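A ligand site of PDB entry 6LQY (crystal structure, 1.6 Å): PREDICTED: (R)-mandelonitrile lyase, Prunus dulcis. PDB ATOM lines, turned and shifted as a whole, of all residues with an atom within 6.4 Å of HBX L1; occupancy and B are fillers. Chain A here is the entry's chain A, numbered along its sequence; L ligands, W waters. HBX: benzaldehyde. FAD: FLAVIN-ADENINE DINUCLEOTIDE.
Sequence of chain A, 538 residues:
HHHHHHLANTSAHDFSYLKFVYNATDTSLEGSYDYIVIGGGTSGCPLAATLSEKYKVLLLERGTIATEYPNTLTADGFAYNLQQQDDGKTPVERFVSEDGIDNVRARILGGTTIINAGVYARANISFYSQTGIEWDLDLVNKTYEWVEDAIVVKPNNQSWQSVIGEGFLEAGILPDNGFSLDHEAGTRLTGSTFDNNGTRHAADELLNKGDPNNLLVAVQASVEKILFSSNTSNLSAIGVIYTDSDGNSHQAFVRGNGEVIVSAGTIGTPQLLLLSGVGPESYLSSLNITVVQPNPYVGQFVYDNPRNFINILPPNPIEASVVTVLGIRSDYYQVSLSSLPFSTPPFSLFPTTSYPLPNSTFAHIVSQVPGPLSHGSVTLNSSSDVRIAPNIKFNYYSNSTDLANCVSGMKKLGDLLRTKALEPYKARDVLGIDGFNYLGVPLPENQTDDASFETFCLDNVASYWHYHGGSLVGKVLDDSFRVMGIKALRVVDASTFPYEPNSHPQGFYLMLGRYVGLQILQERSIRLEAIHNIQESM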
ATOM      1  N   PHE A  78      11.905  14.379 -19.958  1.00  0.00           N
ATOM      2  CA  PHE A  78      13.258  14.709 -20.416  1.00  0.00           C
ATOM      3  C   PHE A  78      13.240  15.847 -21.423  1.00  0.00           C
ATOM      4  O   PHE A  78      13.962  16.843 -21.266  1.00  0.00           O
ATOM      5  CB  PHE A  78      13.915  13.467 -21.033  1.00  0.00           C
ATOM      6  CG  PHE A  78      15.215  13.748 -21.735  1.00  0.00           C
ATOM      7  CD1 PHE A  78      16.368  13.967 -21.011  1.00  0.00           C
ATOM      8  CD2 PHE A  78      15.280  13.786 -23.123  1.00  0.00           C
ATOM      9  CE1 PHE A  78      17.577  14.231 -21.652  1.00  0.00           C
ATOM     10  CE2 PHE A  78      16.483  14.045 -23.769  1.00  0.00           C
ATOM     11  CZ  PHE A  78      17.635  14.267 -23.028  1.00  0.00           C
ATOM     12  N   ALA A 117      19.934  11.981 -19.671  1.00  0.00           N
ATOM     13  CA  ALA A 117      19.196  10.912 -20.345  1.00  0.00           C
ATOM     14  C   ALA A 117      19.209   9.598 -19.554  1.00  0.00           C
ATOM     15  O   ALA A 117      18.716   8.576 -20.056  1.00  0.00           O
ATOM     16  CB  ALA A 117      19.746  10.709 -21.767  1.00  0.00           C
ATOM     17  N   VAL A 119      21.371   7.284 -18.690  1.00  0.00           N
ATOM     18  CA  VAL A 119      22.151   6.095 -18.997  1.00  0.00           C
ATOM     19  C   VAL A 119      23.216   5.901 -17.922  1.00  0.00           C
ATOM     20  O   VAL A 119      23.951   6.840 -17.587  1.00  0.00           O
ATOM     21  CB  VAL A 119      22.798   6.218 -20.387  1.00  0.00           C
ATOM     22  CG1 VAL A 119      23.511   4.913 -20.753  1.00  0.00           C
ATOM     23  CG2 VAL A 119      21.760   6.583 -21.415  1.00  0.00           C
ATOM     24  N   ARG A 307      28.881  14.399 -31.041  1.00  0.00           N
ATOM     25  CA  ARG A 307      27.740  13.550 -31.367  1.00  0.00           C
ATOM     26  C   ARG A 307      27.390  13.758 -32.833  1.00  0.00           C
ATOM     27  O   ARG A 307      27.217  14.893 -33.271  1.00  0.00           O
ATOM     28  CB  ARG A 307      26.523  13.885 -30.486  1.00  0.00           C
ATOM     29  CG  ARG A 307      25.219  13.176 -30.886  1.00  0.00           C
ATOM     30  CD  ARG A 307      24.158  13.228 -29.789  1.00  0.00           C
ATOM     31  NE  ARG A 307      23.965  14.587 -29.323  1.00  0.00           N
ATOM     32  CZ  ARG A 307      22.952  15.376 -29.650  1.00  0.00           C
ATOM     33  NH1 ARG A 307      21.985  14.922 -30.445  1.00  0.00           N
ATOM     34  NH2 ARG A 307      22.912  16.619 -29.210  1.00  0.00           N
ATOM     35  N   VAL A 323      17.212   5.738 -23.557  1.00  0.00           N
ATOM     36  CA  VAL A 323      18.370   4.988 -24.038  1.00  0.00           C
ATOM     37  C   VAL A 323      18.821   3.997 -22.989  1.00  0.00           C
ATOM     38  O   VAL A 323      19.094   4.356 -21.838  1.00  0.00           O
ATOM     39  CB  VAL A 323      19.499   5.947 -24.415  1.00  0.00           C
ATOM     40  CG1 VAL A 323      20.765   5.179 -24.731  1.00  0.00           C
ATOM     41  CG2 VAL A 323      19.080   6.818 -25.591  1.00  0.00           C
ATOM     42  N   VAL A 335      24.196   4.638 -29.830  1.00  0.00           N
ATOM     43  CA  VAL A 335      22.891   4.407 -29.203  1.00  0.00           C
ATOM     44  C   VAL A 335      21.802   4.929 -30.124  1.00  0.00           C
ATOM     45  O   VAL A 335      22.091   5.534 -31.173  1.00  0.00           O
ATOM     46  CB  VAL A 335      22.753   5.126 -27.847  1.00  0.00           C
ATOM     47  CG1 VAL A 335      23.872   4.736 -26.876  1.00  0.00           C
ATOM     48  CG2 VAL A 335      22.700   6.648 -28.062  1.00  0.00           C
ATOM     49  N   LEU A 337      17.809   6.963 -29.581  1.00  0.00           N
ATOM     50  CA  LEU A 337      16.650   7.440 -28.847  1.00  0.00           C
ATOM     51  C   LEU A 337      15.459   7.464 -29.795  1.00  0.00           C
ATOM     52  O   LEU A 337      15.585   7.913 -30.932  1.00  0.00           O
ATOM     53  CB  LEU A 337      16.921   8.850 -28.308  1.00  0.00           C
ATOM     54  CG  LEU A 337      15.761   9.626 -27.708  1.00  0.00           C
ATOM     55  CD1 LEU A 337      15.609   9.233 -26.270  1.00  0.00           C
ATOM     56  CD2 LEU A 337      16.025  11.106 -27.826  1.00  0.00           C
ATOM     57  N   LEU A 349      19.294  19.267 -28.531  1.00  0.00           N
ATOM     58  CA  LEU A 349      19.153  17.971 -29.181  1.00  0.00           C
ATOM     59  C   LEU A 349      19.698  18.041 -30.596  1.00  0.00           C
ATOM     60  O   LEU A 349      20.455  17.170 -31.030  1.00  0.00           O
ATOM     61  CB  LEU A 349      17.690  17.521 -29.178  1.00  0.00           C
ATOM     62  CG  LEU A 349      17.426  16.186 -29.881  1.00  0.00           C
ATOM     63  CD1 LEU A 349      18.071  15.022 -29.116  1.00  0.00           C
ATOM     64  CD2 LEU A 349      15.920  15.959 -30.049  1.00  0.00           C
ATOM     65  N   HIS A 364      16.305   8.807 -33.403  1.00  0.00           N
ATOM     66  CA  HIS A 364      17.555   9.556 -33.438  1.00  0.00           C
ATOM     67  C   HIS A 364      18.662   8.523 -33.235  1.00  0.00           C
ATOM     68  O   HIS A 364      18.731   7.897 -32.169  1.00  0.00           O
ATOM     69  CB  HIS A 364      17.476  10.625 -32.337  1.00  0.00           C
ATOM     70  CG  HIS A 364      18.670  11.509 -32.188  1.00  0.00           C
ATOM     71  ND1 HIS A 364      19.055  12.448 -33.129  1.00  0.00           N
ATOM     72  CD2 HIS A 364      19.484  11.708 -31.124  1.00  0.00           C
ATOM     73  CE1 HIS A 364      20.106  13.127 -32.680  1.00  0.00           C
ATOM     74  NE2 HIS A 364      20.377  12.692 -31.456  1.00  0.00           N
ATOM     75  N   VAL A 366      22.640   7.480 -33.231  1.00  0.00           N
ATOM     76  CA  VAL A 366      23.708   8.354 -32.753  1.00  0.00           C
ATOM     77  C   VAL A 366      25.029   7.610 -32.631  1.00  0.00           C
ATOM     78  O   VAL A 366      25.064   6.440 -32.254  1.00  0.00           O
ATOM     79  CB  VAL A 366      23.306   8.947 -31.380  1.00  0.00           C
ATOM     80  CG1 VAL A 366      24.430   9.691 -30.755  1.00  0.00           C
ATOM     81  CG2 VAL A 366      22.117   9.868 -31.543  1.00  0.00           C
ATOM     82  N   GLN A 368      29.157   8.456 -31.022  1.00  0.00           N
ATOM     83  CA  GLN A 368      29.986   9.308 -30.189  1.00  0.00           C
ATOM     84  C   GLN A 368      31.452   9.050 -30.504  1.00  0.00           C
ATOM     85  O   GLN A 368      31.882   7.890 -30.534  1.00  0.00           O
ATOM     86  CB  GLN A 368      29.716   9.037 -28.697  1.00  0.00           C
ATOM     87  CG  GLN A 368      30.474   9.974 -27.766  1.00  0.00           C
ATOM     88  CD  GLN A 368      30.272   9.664 -26.276  1.00  0.00           C
ATOM     89  OE1 GLN A 368      29.443   8.827 -25.896  1.00  0.00           O
ATOM     90  NE2 GLN A 368      31.024  10.355 -25.434  1.00  0.00           N
ATOM     91  N   TYR A 464      27.613  15.844 -27.539  1.00  0.00           N
ATOM     92  CA  TYR A 464      27.086  14.680 -26.819  1.00  0.00           C
ATOM     93  C   TYR A 464      26.693  15.027 -25.389  1.00  0.00           C
ATOM     94  O   TYR A 464      26.102  14.161 -24.716  1.00  0.00           O
ATOM     95  CB  TYR A 464      28.078  13.511 -26.814  1.00  0.00           C
ATOM     96  CG  TYR A 464      27.339  12.182 -26.896  1.00  0.00           C
ATOM     97  CD1 TYR A 464      26.741  11.614 -25.784  1.00  0.00           C
ATOM     98  CD2 TYR A 464      27.185  11.528 -28.124  1.00  0.00           C
ATOM     99  CE1 TYR A 464      26.037  10.435 -25.867  1.00  0.00           C
ATOM    100  CE2 TYR A 464      26.474  10.343 -28.212  1.00  0.00           C
ATOM    101  CZ  TYR A 464      25.903   9.806 -27.088  1.00  0.00           C
ATOM    102  OH  TYR A 464      25.169   8.635 -27.161  1.00  0.00           O
ATOM    103  N   TRP A 465      27.006  16.229 -24.922  1.00  0.00           N
ATOM    104  CA  TRP A 465      26.711  16.738 -23.595  1.00  0.00           C
ATOM    105  C   TRP A 465      27.675  16.178 -22.563  1.00  0.00           C
ATOM    106  O   TRP A 465      27.510  16.446 -21.347  1.00  0.00           O
ATOM    107  CB  TRP A 465      25.280  16.409 -23.157  1.00  0.00           C
ATOM    108  CG  TRP A 465      24.174  16.961 -24.007  1.00  0.00           C
ATOM    109  CD1 TRP A 465      24.001  18.256 -24.366  1.00  0.00           C
ATOM    110  CD2 TRP A 465      23.049  16.239 -24.531  1.00  0.00           C
ATOM    111  NE1 TRP A 465      22.850  18.394 -25.130  1.00  0.00           N
ATOM    112  CE2 TRP A 465      22.249  17.162 -25.230  1.00  0.00           C
ATOM    113  CE3 TRP A 465      22.651  14.902 -24.486  1.00  0.00           C
ATOM    114  CZ2 TRP A 465      21.076  16.793 -25.888  1.00  0.00           C
ATOM    115  CZ3 TRP A 465      21.478  14.526 -25.137  1.00  0.00           C
ATOM    116  CH2 TRP A 465      20.705  15.469 -25.834  1.00  0.00           C
ATOM    117  N   HIS A 466      28.690  15.436 -22.983  1.00  0.00           N
ATOM    118  CA  HIS A 466      29.608  14.763 -22.064  1.00  0.00           C
ATOM    119  C   HIS A 466      30.923  15.501 -21.965  1.00  0.00           C
ATOM    120  O   HIS A 466      32.003  14.902 -21.919  1.00  0.00           O
ATOM    121  CB  HIS A 466      29.823  13.321 -22.499  1.00  0.00           C
ATOM    122  CG  HIS A 466      28.583  12.472 -22.461  1.00  0.00           C
ATOM    123  ND1 HIS A 466      28.597  11.133 -22.810  1.00  0.00           N
ATOM    124  CD2 HIS A 466      27.313  12.759 -22.096  1.00  0.00           C
ATOM    125  CE1 HIS A 466      27.372  10.644 -22.688  1.00  0.00           C
ATOM    126  NE2 HIS A 466      26.578  11.604 -22.250  1.00  0.00           N
ATOM    127  N   SER A 503      31.292   5.524 -22.292  1.00  0.00           N
ATOM    128  CA  SER A 503      30.378   6.223 -23.188  1.00  0.00           C
ATOM    129  C   SER A 503      29.443   7.179 -22.468  1.00  0.00           C
ATOM    130  O   SER A 503      28.927   8.113 -23.088  1.00  0.00           O
ATOM    131  CB  SER A 503      29.536   5.211 -23.975  1.00  0.00           C
ATOM    132  OG  SER A 503      28.746   4.421 -23.080  1.00  0.00           O
ATOM    133  N   HIS A 504      29.204   6.956 -21.180  1.00  0.00           N
ATOM    134  CA  HIS A 504      28.198   7.684 -20.420  1.00  0.00           C
ATOM    135  C   HIS A 504      28.780   7.869 -19.020  1.00  0.00           C
ATOM    136  O   HIS A 504      28.764   6.930 -18.209  1.00  0.00           O
ATOM    137  CB  HIS A 504      26.863   6.940 -20.399  1.00  0.00           C
ATOM    138  CG  HIS A 504      26.181   6.917 -21.735  1.00  0.00           C
ATOM    139  ND1 HIS A 504      26.487   5.995 -22.721  1.00  0.00           N
ATOM    140  CD2 HIS A 504      25.249   7.737 -22.273  1.00  0.00           C
ATOM    141  CE1 HIS A 504      25.759   6.238 -23.795  1.00  0.00           C
ATOM    142  NE2 HIS A 504      24.991   7.290 -23.547  1.00  0.00           N
HETATM  143  C1' HBX L   1      22.409   9.316 -24.842  1.00  0.00           C
HETATM  144  O1' HBX L   1      23.304   8.635 -25.195  1.00  0.00           O
HETATM  145  C1  HBX L   1      21.628  10.185 -25.729  1.00  0.00           C
HETATM  146  C2  HBX L   1      22.175  10.607 -26.930  1.00  0.00           C
HETATM  147  C3  HBX L   1      21.461  11.449 -27.752  1.00  0.00           C
HETATM  148  C4  HBX L   1      20.203  11.846 -27.410  1.00  0.00           C
HETATM  149  C5  HBX L   1      19.654  11.437 -26.224  1.00  0.00           C
HETATM  150  C6  HBX L   1      20.367  10.609 -25.376  1.00  0.00           C
HETATM  151  PA  FAD L   2      27.083  18.857 -12.575  1.00  0.00           P
HETATM  152  O1A FAD L   2      26.518  19.771 -13.563  1.00  0.00           O
HETATM  153  O2A FAD L   2      26.355  17.631 -12.276  1.00  0.00           O
HETATM  154  O5B FAD L   2      27.266  19.642 -11.214  1.00  0.00           O
HETATM  155  C5B FAD L   2      27.750  20.977 -11.103  1.00  0.00           C
HETATM  156  C4B FAD L   2      26.854  21.745 -10.166  1.00  0.00           C
HETATM  157  O4B FAD L   2      27.462  22.978  -9.725  1.00  0.00           O
HETATM  158  C3B FAD L   2      25.501  22.146 -10.765  1.00  0.00           C
HETATM  159  O3B FAD L   2      24.440  21.670  -9.964  1.00  0.00           O
HETATM  160  C2B FAD L   2      25.562  23.669 -10.826  1.00  0.00           C
HETATM  161  O2B FAD L   2      24.303  24.279 -10.724  1.00  0.00           O
HETATM  162  C1B FAD L   2      26.505  23.999  -9.680  1.00  0.00           C
HETATM  163  N9A FAD L   2      27.218  25.236  -9.763  1.00  0.00           N
HETATM  164  C8A FAD L   2      27.962  25.685 -10.806  1.00  0.00           C
HETATM  165  N7A FAD L   2      28.588  26.796 -10.574  1.00  0.00           N
HETATM  166  C5A FAD L   2      28.248  27.106  -9.276  1.00  0.00           C
HETATM  167  C6A FAD L   2      28.580  28.185  -8.436  1.00  0.00           C
HETATM  168  N6A FAD L   2      29.389  29.156  -8.785  1.00  0.00           N
HETATM  169  N1A FAD L   2      28.043  28.179  -7.193  1.00  0.00           N
HETATM  170  C2A FAD L   2      27.236  27.191  -6.846  1.00  0.00           C
HETATM  171  N3A FAD L   2      26.867  26.126  -7.549  1.00  0.00           N
HETATM  172  C4A FAD L   2      27.403  26.145  -8.765  1.00  0.00           C
HETATM  173  N1  FAD L   2      25.884  11.131 -18.740  1.00  0.00           N
HETATM  174  C2  FAD L   2      25.544   9.851 -18.594  1.00  0.00           C
HETATM  175  O2  FAD L   2      26.298   9.037 -18.090  1.00  0.00           O
HETATM  176  N3  FAD L   2      24.352   9.381 -19.042  1.00  0.00           N
HETATM  177  C4  FAD L   2      23.466  10.173 -19.733  1.00  0.00           C
HETATM  178  O4  FAD L   2      22.429   9.712 -20.091  1.00  0.00           O
HETATM  179  C4X FAD L   2      23.768  11.549 -19.841  1.00  0.00           C
HETATM  180  N5  FAD L   2      22.924  12.342 -20.424  1.00  0.00           N
HETATM  181  C5X FAD L   2      23.188  13.672 -20.422  1.00  0.00           C
HETATM  182  C6  FAD L   2      22.243  14.560 -20.963  1.00  0.00           C
HETATM  183  C7  FAD L   2      22.404  15.925 -20.906  1.00  0.00           C
HETATM  184  C7M FAD L   2      21.355  16.852 -21.457  1.00  0.00           C
HETATM  185  C8  FAD L   2      23.585  16.431 -20.342  1.00  0.00           C
HETATM  186  C8M FAD L   2      23.806  17.918 -20.286  1.00  0.00           C
HETATM  187  C9  FAD L   2      24.570  15.572 -19.913  1.00  0.00           C
HETATM  188  C9A FAD L   2      24.375  14.193 -19.885  1.00  0.00           C
HETATM  189  N10 FAD L   2      25.321  13.297 -19.378  1.00  0.00           N
HETATM  190  C10 FAD L   2      25.036  11.961 -19.302  1.00  0.00           C
HETATM  191  C1' FAD L   2      26.596  13.786 -18.838  1.00  0.00           C
HETATM  192  C2' FAD L   2      26.706  13.703 -17.343  1.00  0.00           C
HETATM  193  O2' FAD L   2      25.446  13.819 -16.783  1.00  0.00           O
HETATM  194  C3' FAD L   2      27.636  14.837 -16.887  1.00  0.00           C
HETATM  195  O3' FAD L   2      28.862  14.782 -17.537  1.00  0.00           O
HETATM  196  C4' FAD L   2      27.905  14.880 -15.386  1.00  0.00           C
HETATM  197  O4' FAD L   2      26.641  14.808 -14.739  1.00  0.00           O
HETATM  198  C5' FAD L   2      28.663  16.102 -14.927  1.00  0.00           C
HETATM  199  O5' FAD L   2      28.822  16.096 -13.489  1.00  0.00           O
HETATM  200  P   FAD L   2      29.518  17.306 -12.723  1.00  0.00           P
HETATM  201  O1P FAD L   2      29.482  17.036 -11.279  1.00  0.00           O
HETATM  202  O2P FAD L   2      30.785  17.562 -13.391  1.00  0.00           O
HETATM  203  O3P FAD L   2      28.531  18.489 -13.043  1.00  0.00           O
HETATM  204  O   HOH W   1      23.821  11.150 -23.184  1.00  0.00           O
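The backbone NH (N) of Ala 117 lies within hydrogen-bond range of a nitrogen (N5) of FAD L2 (3.1 Å). OH of Tyr 464 lies within hydrogen-bond range of O1' of HBX L1, 2.7 Å away. A ring nitrogen (NE2) of His 504 is in hydrogen-bond range of an oxygen (O1') of HBX L1 (2.7 Å). The backbone NH (N) of Val 119 sits at hydrogen-bond distance from an oxygen (O4) of FAD L2. N3 of FAD L2 sits at hydrogen-bond distance from O of Val 119 (3.0 Å).
Residues that only touch HBX L1: Ala 117 (3.7 Å), Arg 307 (3.8 Å), Val 335 (3.5 Å), Leu 337 (3.98 Å), His 364 (3.8 Å) and Trp 465 (3.7 Å). Within 4 Å of HBX L1: Ala 117, Arg 307, Val 335, Leu 337, His 364, Tyr 464, Trp 465 and His 504. The nearest printed residue that does not touch HBX L1 is Val 323 (4.01 Å).
Water W1 lies within hydrogen-bond range of NE2 of His 466, N5 of FAD L2 and O1' of HBX L1.
A ring nitrogen (NE2) of His 364 is in hydrogen-bond range of the guanidinium group of Arg 307, at 2.9 Å. O of Leu 349 is in hydrogen-bond range of NH1 of Arg 307. The backbone carbonyl oxygen (O) of Val 335 is in hydrogen-bond range of the backbone NH (N) of Val 366. ND1 of His 504 is in hydrogen-bond range of OG of Ser 503 (2.8 Å). O of Leu 337 is in hydrogen-bond range of N of His 364, at 2.7 Å.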
